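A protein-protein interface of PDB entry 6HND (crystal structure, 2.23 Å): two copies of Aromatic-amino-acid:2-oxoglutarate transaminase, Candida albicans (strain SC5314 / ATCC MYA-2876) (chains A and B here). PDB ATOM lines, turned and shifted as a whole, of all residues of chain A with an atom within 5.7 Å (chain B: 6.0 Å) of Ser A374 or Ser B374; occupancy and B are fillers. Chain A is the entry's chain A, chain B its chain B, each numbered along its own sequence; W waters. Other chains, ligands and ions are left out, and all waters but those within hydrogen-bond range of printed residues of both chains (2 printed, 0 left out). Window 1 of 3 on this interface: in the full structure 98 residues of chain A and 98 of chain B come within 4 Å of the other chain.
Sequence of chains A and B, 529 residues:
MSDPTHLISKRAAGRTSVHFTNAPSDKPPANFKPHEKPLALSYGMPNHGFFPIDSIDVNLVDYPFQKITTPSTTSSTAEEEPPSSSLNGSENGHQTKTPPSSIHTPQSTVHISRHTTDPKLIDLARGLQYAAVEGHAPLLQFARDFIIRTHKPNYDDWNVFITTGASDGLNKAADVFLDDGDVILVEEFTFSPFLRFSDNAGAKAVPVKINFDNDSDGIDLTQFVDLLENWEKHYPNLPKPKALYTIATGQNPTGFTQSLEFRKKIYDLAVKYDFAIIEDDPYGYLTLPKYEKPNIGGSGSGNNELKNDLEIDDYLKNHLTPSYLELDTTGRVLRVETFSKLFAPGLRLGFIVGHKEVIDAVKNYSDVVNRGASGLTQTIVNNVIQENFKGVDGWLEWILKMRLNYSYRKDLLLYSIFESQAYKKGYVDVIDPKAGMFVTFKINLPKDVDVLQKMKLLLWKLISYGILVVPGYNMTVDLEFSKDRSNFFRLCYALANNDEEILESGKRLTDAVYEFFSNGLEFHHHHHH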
ATOM      1  N   THR A 164      26.413 -24.403 -19.653  1.00  0.00           N
ATOM      2  CA  THR A 164      25.677 -25.410 -20.454  1.00  0.00           C
ATOM      3  C   THR A 164      26.326 -26.784 -20.316  1.00  0.00           C
ATOM      4  O   THR A 164      26.085 -27.592 -21.201  1.00  0.00           O
ATOM      5  CB  THR A 164      25.504 -24.939 -21.899  1.00  0.00           C
ATOM      6  OG1 THR A 164      26.752 -24.750 -22.573  1.00  0.00           O
ATOM      7  CG2 THR A 164      24.701 -23.657 -21.912  1.00  0.00           C
ATOM      8  N   GLY A 346      21.530 -34.459 -21.514  1.00  0.00           N
ATOM      9  CA  GLY A 346      20.777 -33.721 -22.539  1.00  0.00           C
ATOM     10  C   GLY A 346      20.231 -32.434 -21.986  1.00  0.00           C
ATOM     11  O   GLY A 346      19.582 -31.688 -22.744  1.00  0.00           O
ATOM     12  N   LEU A 347      20.437 -32.182 -20.691  1.00  0.00           N
ATOM     13  CA  LEU A 347      20.107 -30.869 -20.084  1.00  0.00           C
ATOM     14  C   LEU A 347      20.982 -29.780 -20.722  1.00  0.00           C
ATOM     15  O   LEU A 347      20.457 -28.711 -21.002  1.00  0.00           O
ATOM     16  CB  LEU A 347      20.351 -30.915 -18.582  1.00  0.00           C
ATOM     17  CG  LEU A 347      19.504 -31.900 -17.787  1.00  0.00           C
ATOM     18  CD1 LEU A 347      20.035 -31.961 -16.369  1.00  0.00           C
ATOM     19  CD2 LEU A 347      18.044 -31.490 -17.778  1.00  0.00           C
ATOM     20  N   ARG A 348      22.270 -30.061 -20.948  1.00  0.00           N
ATOM     21  CA  ARG A 348      23.267 -29.034 -21.316  1.00  0.00           C
ATOM     22  C   ARG A 348      23.219 -27.970 -20.216  1.00  0.00           C
ATOM     23  O   ARG A 348      22.886 -26.791 -20.494  1.00  0.00           O
ATOM     24  CB  ARG A 348      23.001 -28.442 -22.708  1.00  0.00           C
ATOM     25  CG  ARG A 348      23.078 -29.430 -23.864  1.00  0.00           C
ATOM     26  CD  ARG A 348      24.459 -30.010 -24.139  1.00  0.00           C
ATOM     27  NE  ARG A 348      24.778 -31.098 -23.242  1.00  0.00           N
ATOM     28  CZ  ARG A 348      26.007 -31.458 -22.871  1.00  0.00           C
ATOM     29  NH1 ARG A 348      27.077 -30.831 -23.334  1.00  0.00           N
ATOM     30  NH2 ARG A 348      26.161 -32.441 -22.002  1.00  0.00           N
ATOM     31  N   LEU A 349      23.500 -28.389 -18.986  1.00  0.00           N
ATOM     32  CA  LEU A 349      23.423 -27.503 -17.802  1.00  0.00           C
ATOM     33  C   LEU A 349      24.516 -27.877 -16.817  1.00  0.00           C
ATOM     34  O   LEU A 349      24.727 -29.070 -16.601  1.00  0.00           O
ATOM     35  CB  LEU A 349      22.033 -27.635 -17.173  1.00  0.00           C
ATOM     36  CG  LEU A 349      21.709 -26.561 -16.139  1.00  0.00           C
ATOM     37  CD1 LEU A 349      21.683 -25.215 -16.816  1.00  0.00           C
ATOM     38  CD2 LEU A 349      20.397 -26.872 -15.430  1.00  0.00           C
ATOM     39  N   GLY A 372      23.754 -17.786 -22.381  1.00  0.00           N
ATOM     40  CA  GLY A 372      22.861 -18.349 -21.347  1.00  0.00           C
ATOM     41  C   GLY A 372      22.458 -19.798 -21.615  1.00  0.00           C
ATOM     42  O   GLY A 372      22.097 -20.141 -22.773  1.00  0.00           O
ATOM     43  N   ALA A 373      22.543 -20.635 -20.581  1.00  0.00           N
ATOM     44  CA  ALA A 373      21.859 -21.946 -20.521  1.00  0.00           C
ATOM     45  C   ALA A 373      20.351 -21.763 -20.755  1.00  0.00           C
ATOM     46  O   ALA A 373      19.785 -20.777 -20.294  1.00  0.00           O
ATOM     47  CB  ALA A 373      22.130 -22.600 -19.205  1.00  0.00           C
ATOM     48  N   SER A 374      19.742 -22.657 -21.522  1.00  0.00           N
ATOM     49  CA  SER A 374      18.277 -22.680 -21.751  1.00  0.00           C
ATOM     50  C   SER A 374      17.526 -22.304 -20.461  1.00  0.00           C
ATOM     51  O   SER A 374      17.658 -23.014 -19.453  1.00  0.00           O
ATOM     52  CB  SER A 374      17.830 -24.026 -22.273  1.00  0.00           C
ATOM     53  OG  SER A 374      16.450 -23.984 -22.598  1.00  0.00           O
ATOM     54  N   GLY A 375      16.723 -21.244 -20.515  1.00  0.00           N
ATOM     55  CA  GLY A 375      15.857 -20.793 -19.412  1.00  0.00           C
ATOM     56  C   GLY A 375      14.845 -21.844 -19.034  1.00  0.00           C
ATOM     57  O   GLY A 375      14.624 -22.038 -17.840  1.00  0.00           O
ATOM     58  N   LEU A 376      14.260 -22.519 -20.012  1.00  0.00           N
ATOM     59  CA  LEU A 376      13.239 -23.575 -19.772  1.00  0.00           C
ATOM     60  C   LEU A 376      13.888 -24.751 -19.032  1.00  0.00           C
ATOM     61  O   LEU A 376      13.262 -25.296 -18.106  1.00  0.00           O
ATOM     62  CB  LEU A 376      12.671 -24.025 -21.117  1.00  0.00           C
ATOM     63  CG  LEU A 376      11.762 -25.239 -21.059  1.00  0.00           C
ATOM     64  CD1 LEU A 376      10.622 -24.963 -20.111  1.00  0.00           C
ATOM     65  CD2 LEU A 376      11.239 -25.573 -22.453  1.00  0.00           C
ATOM     66  N   THR A 377      15.117 -25.121 -19.411  1.00  0.00           N
ATOM     67  CA  THR A 377      15.893 -26.195 -18.732  1.00  0.00           C
ATOM     68  C   THR A 377      16.223 -25.748 -17.303  1.00  0.00           C
ATOM     69  O   THR A 377      16.000 -26.529 -16.400  1.00  0.00           O
ATOM     70  CB  THR A 377      17.102 -26.599 -19.561  1.00  0.00           C
ATOM     71  OG1 THR A 377      16.563 -27.041 -20.810  1.00  0.00           O
ATOM     72  CG2 THR A 377      17.928 -27.703 -18.940  1.00  0.00           C
ATOM     73  N   GLN A 378      16.660 -24.509 -17.098  1.00  0.00           N
ATOM     74  CA  GLN A 378      16.973 -23.999 -15.739  1.00  0.00           C
ATOM     75  C   GLN A 378      15.705 -24.091 -14.909  1.00  0.00           C
ATOM     76  O   GLN A 378      15.787 -24.480 -13.725  1.00  0.00           O
ATOM     77  CB  GLN A 378      17.463 -22.557 -15.753  1.00  0.00           C
ATOM     78  CG  GLN A 378      18.826 -22.415 -16.380  1.00  0.00           C
ATOM     79  CD  GLN A 378      19.293 -20.997 -16.263  1.00  0.00           C
ATOM     80  OE1 GLN A 378      19.421 -20.480 -15.159  1.00  0.00           O
ATOM     81  NE2 GLN A 378      19.571 -20.384 -17.403  1.00  0.00           N
ATOM     82  N   THR A 379      14.588 -23.728 -15.519  1.00  0.00           N
ATOM     83  CA  THR A 379      13.274 -23.775 -14.853  1.00  0.00           C
ATOM     84  C   THR A 379      13.000 -25.207 -14.376  1.00  0.00           C
ATOM     85  O   THR A 379      12.683 -25.388 -13.194  1.00  0.00           O
ATOM     86  CB  THR A 379      12.187 -23.241 -15.780  1.00  0.00           C
ATOM     87  OG1 THR A 379      12.546 -21.883 -16.075  1.00  0.00           O
ATOM     88  CG2 THR A 379      10.824 -23.371 -15.139  1.00  0.00           C
ATOM     89  N   GLY B 127      16.265 -37.511 -25.746  1.00  0.00           N
ATOM     90  CA  GLY B 127      16.218 -36.058 -25.485  1.00  0.00           C
ATOM     91  C   GLY B 127      17.113 -35.664 -24.323  1.00  0.00           C
ATOM     92  O   GLY B 127      17.754 -34.586 -24.388  1.00  0.00           O
ATOM     93  N   THR B 164      21.477 -21.789 -30.228  1.00  0.00           N
ATOM     94  CA  THR B 164      20.858 -21.387 -28.945  1.00  0.00           C
ATOM     95  C   THR B 164      20.182 -20.016 -29.096  1.00  0.00           C
ATOM     96  O   THR B 164      19.933 -19.390 -28.077  1.00  0.00           O
ATOM     97  CB  THR B 164      21.880 -21.511 -27.812  1.00  0.00           C
ATOM     98  OG1 THR B 164      23.067 -20.742 -28.049  1.00  0.00           O
ATOM     99  CG2 THR B 164      22.267 -22.963 -27.617  1.00  0.00           C
ATOM    100  N   GLY B 346      13.389 -17.461 -23.592  1.00  0.00           N
ATOM    101  CA  GLY B 346      13.927 -18.347 -22.545  1.00  0.00           C
ATOM    102  C   GLY B 346      14.280 -19.727 -23.085  1.00  0.00           C
ATOM    103  O   GLY B 346      14.969 -20.467 -22.367  1.00  0.00           O
ATOM    104  N   LEU B 347      13.847 -20.071 -24.305  1.00  0.00           N
ATOM    105  CA  LEU B 347      14.221 -21.377 -24.902  1.00  0.00           C
ATOM    106  C   LEU B 347      15.742 -21.389 -25.078  1.00  0.00           C
ATOM    107  O   LEU B 347      16.365 -22.454 -24.776  1.00  0.00           O
ATOM    108  CB  LEU B 347      13.556 -21.598 -26.261  1.00  0.00           C
ATOM    109  CG  LEU B 347      12.040 -21.669 -26.340  1.00  0.00           C
ATOM    110  CD1 LEU B 347      11.658 -21.903 -27.781  1.00  0.00           C
ATOM    111  CD2 LEU B 347      11.451 -22.760 -25.450  1.00  0.00           C
ATOM    112  N   ARG B 348      16.298 -20.262 -25.559  1.00  0.00           N
ATOM    113  CA  ARG B 348      17.684 -20.186 -26.099  1.00  0.00           C
ATOM    114  C   ARG B 348      17.808 -21.243 -27.218  1.00  0.00           C
ATOM    115  O   ARG B 348      18.557 -22.207 -27.057  1.00  0.00           O
ATOM    116  CB  ARG B 348      18.720 -20.467 -25.006  1.00  0.00           C
ATOM    117  CG  ARG B 348      18.771 -19.492 -23.842  1.00  0.00           C
ATOM    118  CD  ARG B 348      19.305 -18.141 -24.253  1.00  0.00           C
ATOM    119  NE  ARG B 348      18.214 -17.421 -24.881  1.00  0.00           N
ATOM    120  CZ  ARG B 348      18.346 -16.381 -25.686  1.00  0.00           C
ATOM    121  NH1 ARG B 348      17.248 -15.821 -26.168  1.00  0.00           N
ATOM    122  NH2 ARG B 348      19.545 -15.909 -26.013  1.00  0.00           N
ATOM    123  N   LEU B 349      17.015 -21.105 -28.272  1.00  0.00           N
ATOM    124  CA  LEU B 349      16.903 -22.064 -29.391  1.00  0.00           C
ATOM    125  C   LEU B 349      16.631 -21.304 -30.679  1.00  0.00           C
ATOM    126  O   LEU B 349      15.833 -20.365 -30.661  1.00  0.00           O
ATOM    127  CB  LEU B 349      15.792 -23.092 -29.144  1.00  0.00           C
ATOM    128  CG  LEU B 349      15.880 -24.329 -30.044  1.00  0.00           C
ATOM    129  CD1 LEU B 349      17.050 -25.184 -29.640  1.00  0.00           C
ATOM    130  CD2 LEU B 349      14.595 -25.134 -29.995  1.00  0.00           C
ATOM    131  N   GLY B 372      26.112 -27.582 -28.055  1.00  0.00           N
ATOM    132  CA  GLY B 372      24.731 -28.051 -28.247  1.00  0.00           C
ATOM    133  C   GLY B 372      23.711 -27.183 -27.547  1.00  0.00           C
ATOM    134  O   GLY B 372      23.944 -26.768 -26.367  1.00  0.00           O
ATOM    135  N   ALA B 373      22.616 -26.924 -28.253  1.00  0.00           N
ATOM    136  CA  ALA B 373      21.349 -26.462 -27.659  1.00  0.00           C
ATOM    137  C   ALA B 373      20.836 -27.530 -26.696  1.00  0.00           C
ATOM    138  O   ALA B 373      20.996 -28.715 -26.994  1.00  0.00           O
ATOM    139  CB  ALA B 373      20.338 -26.164 -28.732  1.00  0.00           C
ATOM    140  N   SER B 374      20.258 -27.106 -25.575  1.00  0.00           N
ATOM    141  CA  SER B 374      19.613 -28.009 -24.580  1.00  0.00           C
ATOM    142  C   SER B 374      18.723 -29.044 -25.278  1.00  0.00           C
ATOM    143  O   SER B 374      17.761 -28.651 -25.916  1.00  0.00           O
ATOM    144  CB  SER B 374      18.812 -27.243 -23.578  1.00  0.00           C
ATOM    145  OG  SER B 374      18.402 -28.103 -22.540  1.00  0.00           O
ATOM    146  N   GLY B 375      19.043 -30.323 -25.143  1.00  0.00           N
ATOM    147  CA  GLY B 375      18.235 -31.421 -25.697  1.00  0.00           C
ATOM    148  C   GLY B 375      16.838 -31.418 -25.117  1.00  0.00           C
ATOM    149  O   GLY B 375      15.891 -31.728 -25.866  1.00  0.00           O
ATOM    150  N   LEU B 376      16.698 -31.090 -23.832  1.00  0.00           N
ATOM    151  CA  LEU B 376      15.372 -31.088 -23.150  1.00  0.00           C
ATOM    152  C   LEU B 376      14.516 -30.042 -23.857  1.00  0.00           C
ATOM    153  O   LEU B 376      13.332 -30.282 -24.038  1.00  0.00           O
ATOM    154  CB  LEU B 376      15.529 -30.782 -21.649  1.00  0.00           C
ATOM    155  CG  LEU B 376      14.220 -30.672 -20.860  1.00  0.00           C
ATOM    156  CD1 LEU B 376      13.295 -31.856 -21.123  1.00  0.00           C
ATOM    157  CD2 LEU B 376      14.467 -30.515 -19.366  1.00  0.00           C
ATOM    158  N   THR B 377      15.109 -28.917 -24.247  1.00  0.00           N
ATOM    159  CA  THR B 377      14.371 -27.793 -24.878  1.00  0.00           C
ATOM    160  C   THR B 377      14.026 -28.168 -26.314  1.00  0.00           C
ATOM    161  O   THR B 377      12.882 -27.907 -26.716  1.00  0.00           O
ATOM    162  CB  THR B 377      15.173 -26.500 -24.823  1.00  0.00           C
ATOM    163  OG1 THR B 377      15.316 -26.257 -23.425  1.00  0.00           O
ATOM    164  CG2 THR B 377      14.506 -25.352 -25.557  1.00  0.00           C
ATOM    165  N   GLN B 378      14.994 -28.724 -27.047  1.00  0.00           N
ATOM    166  CA  GLN B 378      14.781 -29.256 -28.415  1.00  0.00           C
ATOM    167  C   GLN B 378      13.627 -30.258 -28.353  1.00  0.00           C
ATOM    168  O   GLN B 378      12.830 -30.284 -29.288  1.00  0.00           O
ATOM    169  CB  GLN B 378      16.022 -29.957 -28.948  1.00  0.00           C
ATOM    170  CG  GLN B 378      17.166 -29.022 -29.281  1.00  0.00           C
ATOM    171  CD  GLN B 378      18.295 -29.763 -29.956  1.00  0.00           C
ATOM    172  OE1 GLN B 378      18.112 -30.354 -31.033  1.00  0.00           O
ATOM    173  NE2 GLN B 378      19.473 -29.722 -29.336  1.00  0.00           N
ATOM    174  N   THR B 379      13.591 -31.080 -27.305  1.00  0.00           N
ATOM    175  CA  THR B 379      12.570 -32.142 -27.121  1.00  0.00           C
ATOM    176  C   THR B 379      11.212 -31.458 -26.947  1.00  0.00           C
ATOM    177  O   THR B 379      10.330 -31.754 -27.748  1.00  0.00           O
ATOM    178  CB  THR B 379      12.942 -33.080 -25.967  1.00  0.00           C
ATOM    179  OG1 THR B 379      14.190 -33.675 -26.309  1.00  0.00           O
ATOM    180  CG2 THR B 379      11.906 -34.152 -25.699  1.00  0.00           C
HETATM  181  O   HOH W   1      23.357 -19.708 -25.333  1.00  0.00           O
HETATM  182  O   HOH W   2      26.394 -25.808 -25.180  1.00  0.00           O
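Gly A346 touches Gly B375, and with the chains exchanged Gly A375 touches Gly B346. Leu A347 touches Ser B374, and with the chains exchanged Ser A374 touches Leu B347. Arg A348 touches Ser B374, and with the chains exchanged Ser A374 touches Arg B348. Thr A377 touches its own counterpart, Thr B377. Of the 20 pairs that touch across the chains among the printed residues, 18 have their exchanged pair printed and touching as well.
OG1 of Thr A379 sits at hydrogen-bond distance from O of Gly A375 (2.7 Å). The side-chain amide nitrogen of Gln A378 lies within hydrogen-bond range of the backbone carbonyl oxygen of Ala A373, 2.9 Å away. The backbone carbonyl oxygen (O) of Ala B373 sits at hydrogen-bond distance from the side-chain amide nitrogen (NE2) of Gln B378 (3.0 Å). The side-chain hydroxyl (OG1) of Thr B379 is in hydrogen-bond range of the backbone carbonyl oxygen (O) of Gly B375 (2.6 Å).
Ser A374 touches just these residues of chain B: Gly B346, Leu B347, Arg B348, Ser B374 and Thr B377. Of chain A, only Gly A346 (3.8 Å), Leu A347 (2.6 Å), Arg A348 (3.8 Å), Ser A374 (3.6 Å) and Thr A377 (2.7 Å) come within 4 Å of Ser B374. Printed residues of chain B within 4 Å of Gly A375: Gly B346. Of the printed residues of chain A, Gly B127 touches Gly A346. Of the printed residues of chain A, Leu B376 touches Gly A346 and Thr A377. Of the printed residues of chain A, Ala B373 touches Arg A348 (3.8 Å). Of the printed residues of chain A, Thr B377 touches Ser A374 (2.7 Å) and Thr A377 (3.0 Å). The nearest printed residue of chain A that does not touch Ser B374 is Leu A349 (6.2 Å). The nearest printed residue of chain B that does not touch Leu A347 is Leu B376 (4.03 Å).
The backbone carbonyl oxygen of Gly B346 is in hydrogen-bond range of the backbone NH of Gly A375 (2.7 Å). The backbone NH (N) of Leu A376 lies within hydrogen-bond range of the backbone carbonyl oxygen (O) of Gly B346 (3.2 Å). The side-chain hydroxyl (OG1) of Thr A377 lies within hydrogen-bond range of the side-chain hydroxyl (OG1) of Thr B377. The side-chain hydroxyl (OG) of Ser A374 is in hydrogen-bond range of the side-chain hydroxyl (OG1) of Thr B377 (2.7 Å). The side-chain hydroxyl (OG1) of Thr A377 is in hydrogen-bond range of the side-chain hydroxyl (OG) of Ser B374, 2.7 Å away. The backbone carbonyl oxygen of Gly A346 sits at hydrogen-bond distance from the backbone NH of Leu B376, 3.1 Å away. The side-chain hydroxyl (OG) of Ser A374 is in hydrogen-bond range of the backbone carbonyl oxygen (O) of Leu B347 (2.7 Å). The backbone carbonyl oxygen (O) of Leu A347 lies within hydrogen-bond range of the side-chain hydroxyl (OG) of Ser B374 (2.6 Å). The backbone carbonyl oxygen (O) of Gly A346 sits at hydrogen-bond distance from the backbone NH (N) of Gly B375 (2.8 Å).
Water W2 lies within hydrogen-bond range of OG1 of Thr A164 (2.8 Å) and O of Gly B372 (2.9 Å). Water W1 bridges O of Gly A372 and OG1 of Thr B164.
CA of Gly A346 touches O of Gly B127, at 3.6 Å. Ser B374 touches Gly A346. Arg A348 touches Gly B372 (CG to O, 3.8 Å). CG of Arg A348 touches O of Ala B373 (3.8 Å). O of Gly A372 touches CG of Arg B348 (3.6 Å). Arg B348 touches Ala A373. O of Gly B346 touches C of Ser A374 (3.7 Å). Arg B348 touches Ser A374. Ser A374 touches Ser B374. CB of Leu B376 touches OG1 of Thr A377 (3.97 Å).
Hydrophobic or aromatic side chains of chain B that line the printed part of chain A: Leu B376. Printed residues of chain A that touch a printed residue of chain B: Gly A346, Leu A347, Arg A348, Gly A372, Ala A373, Ser A374, Gly A375, Leu A376 and Thr A377.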
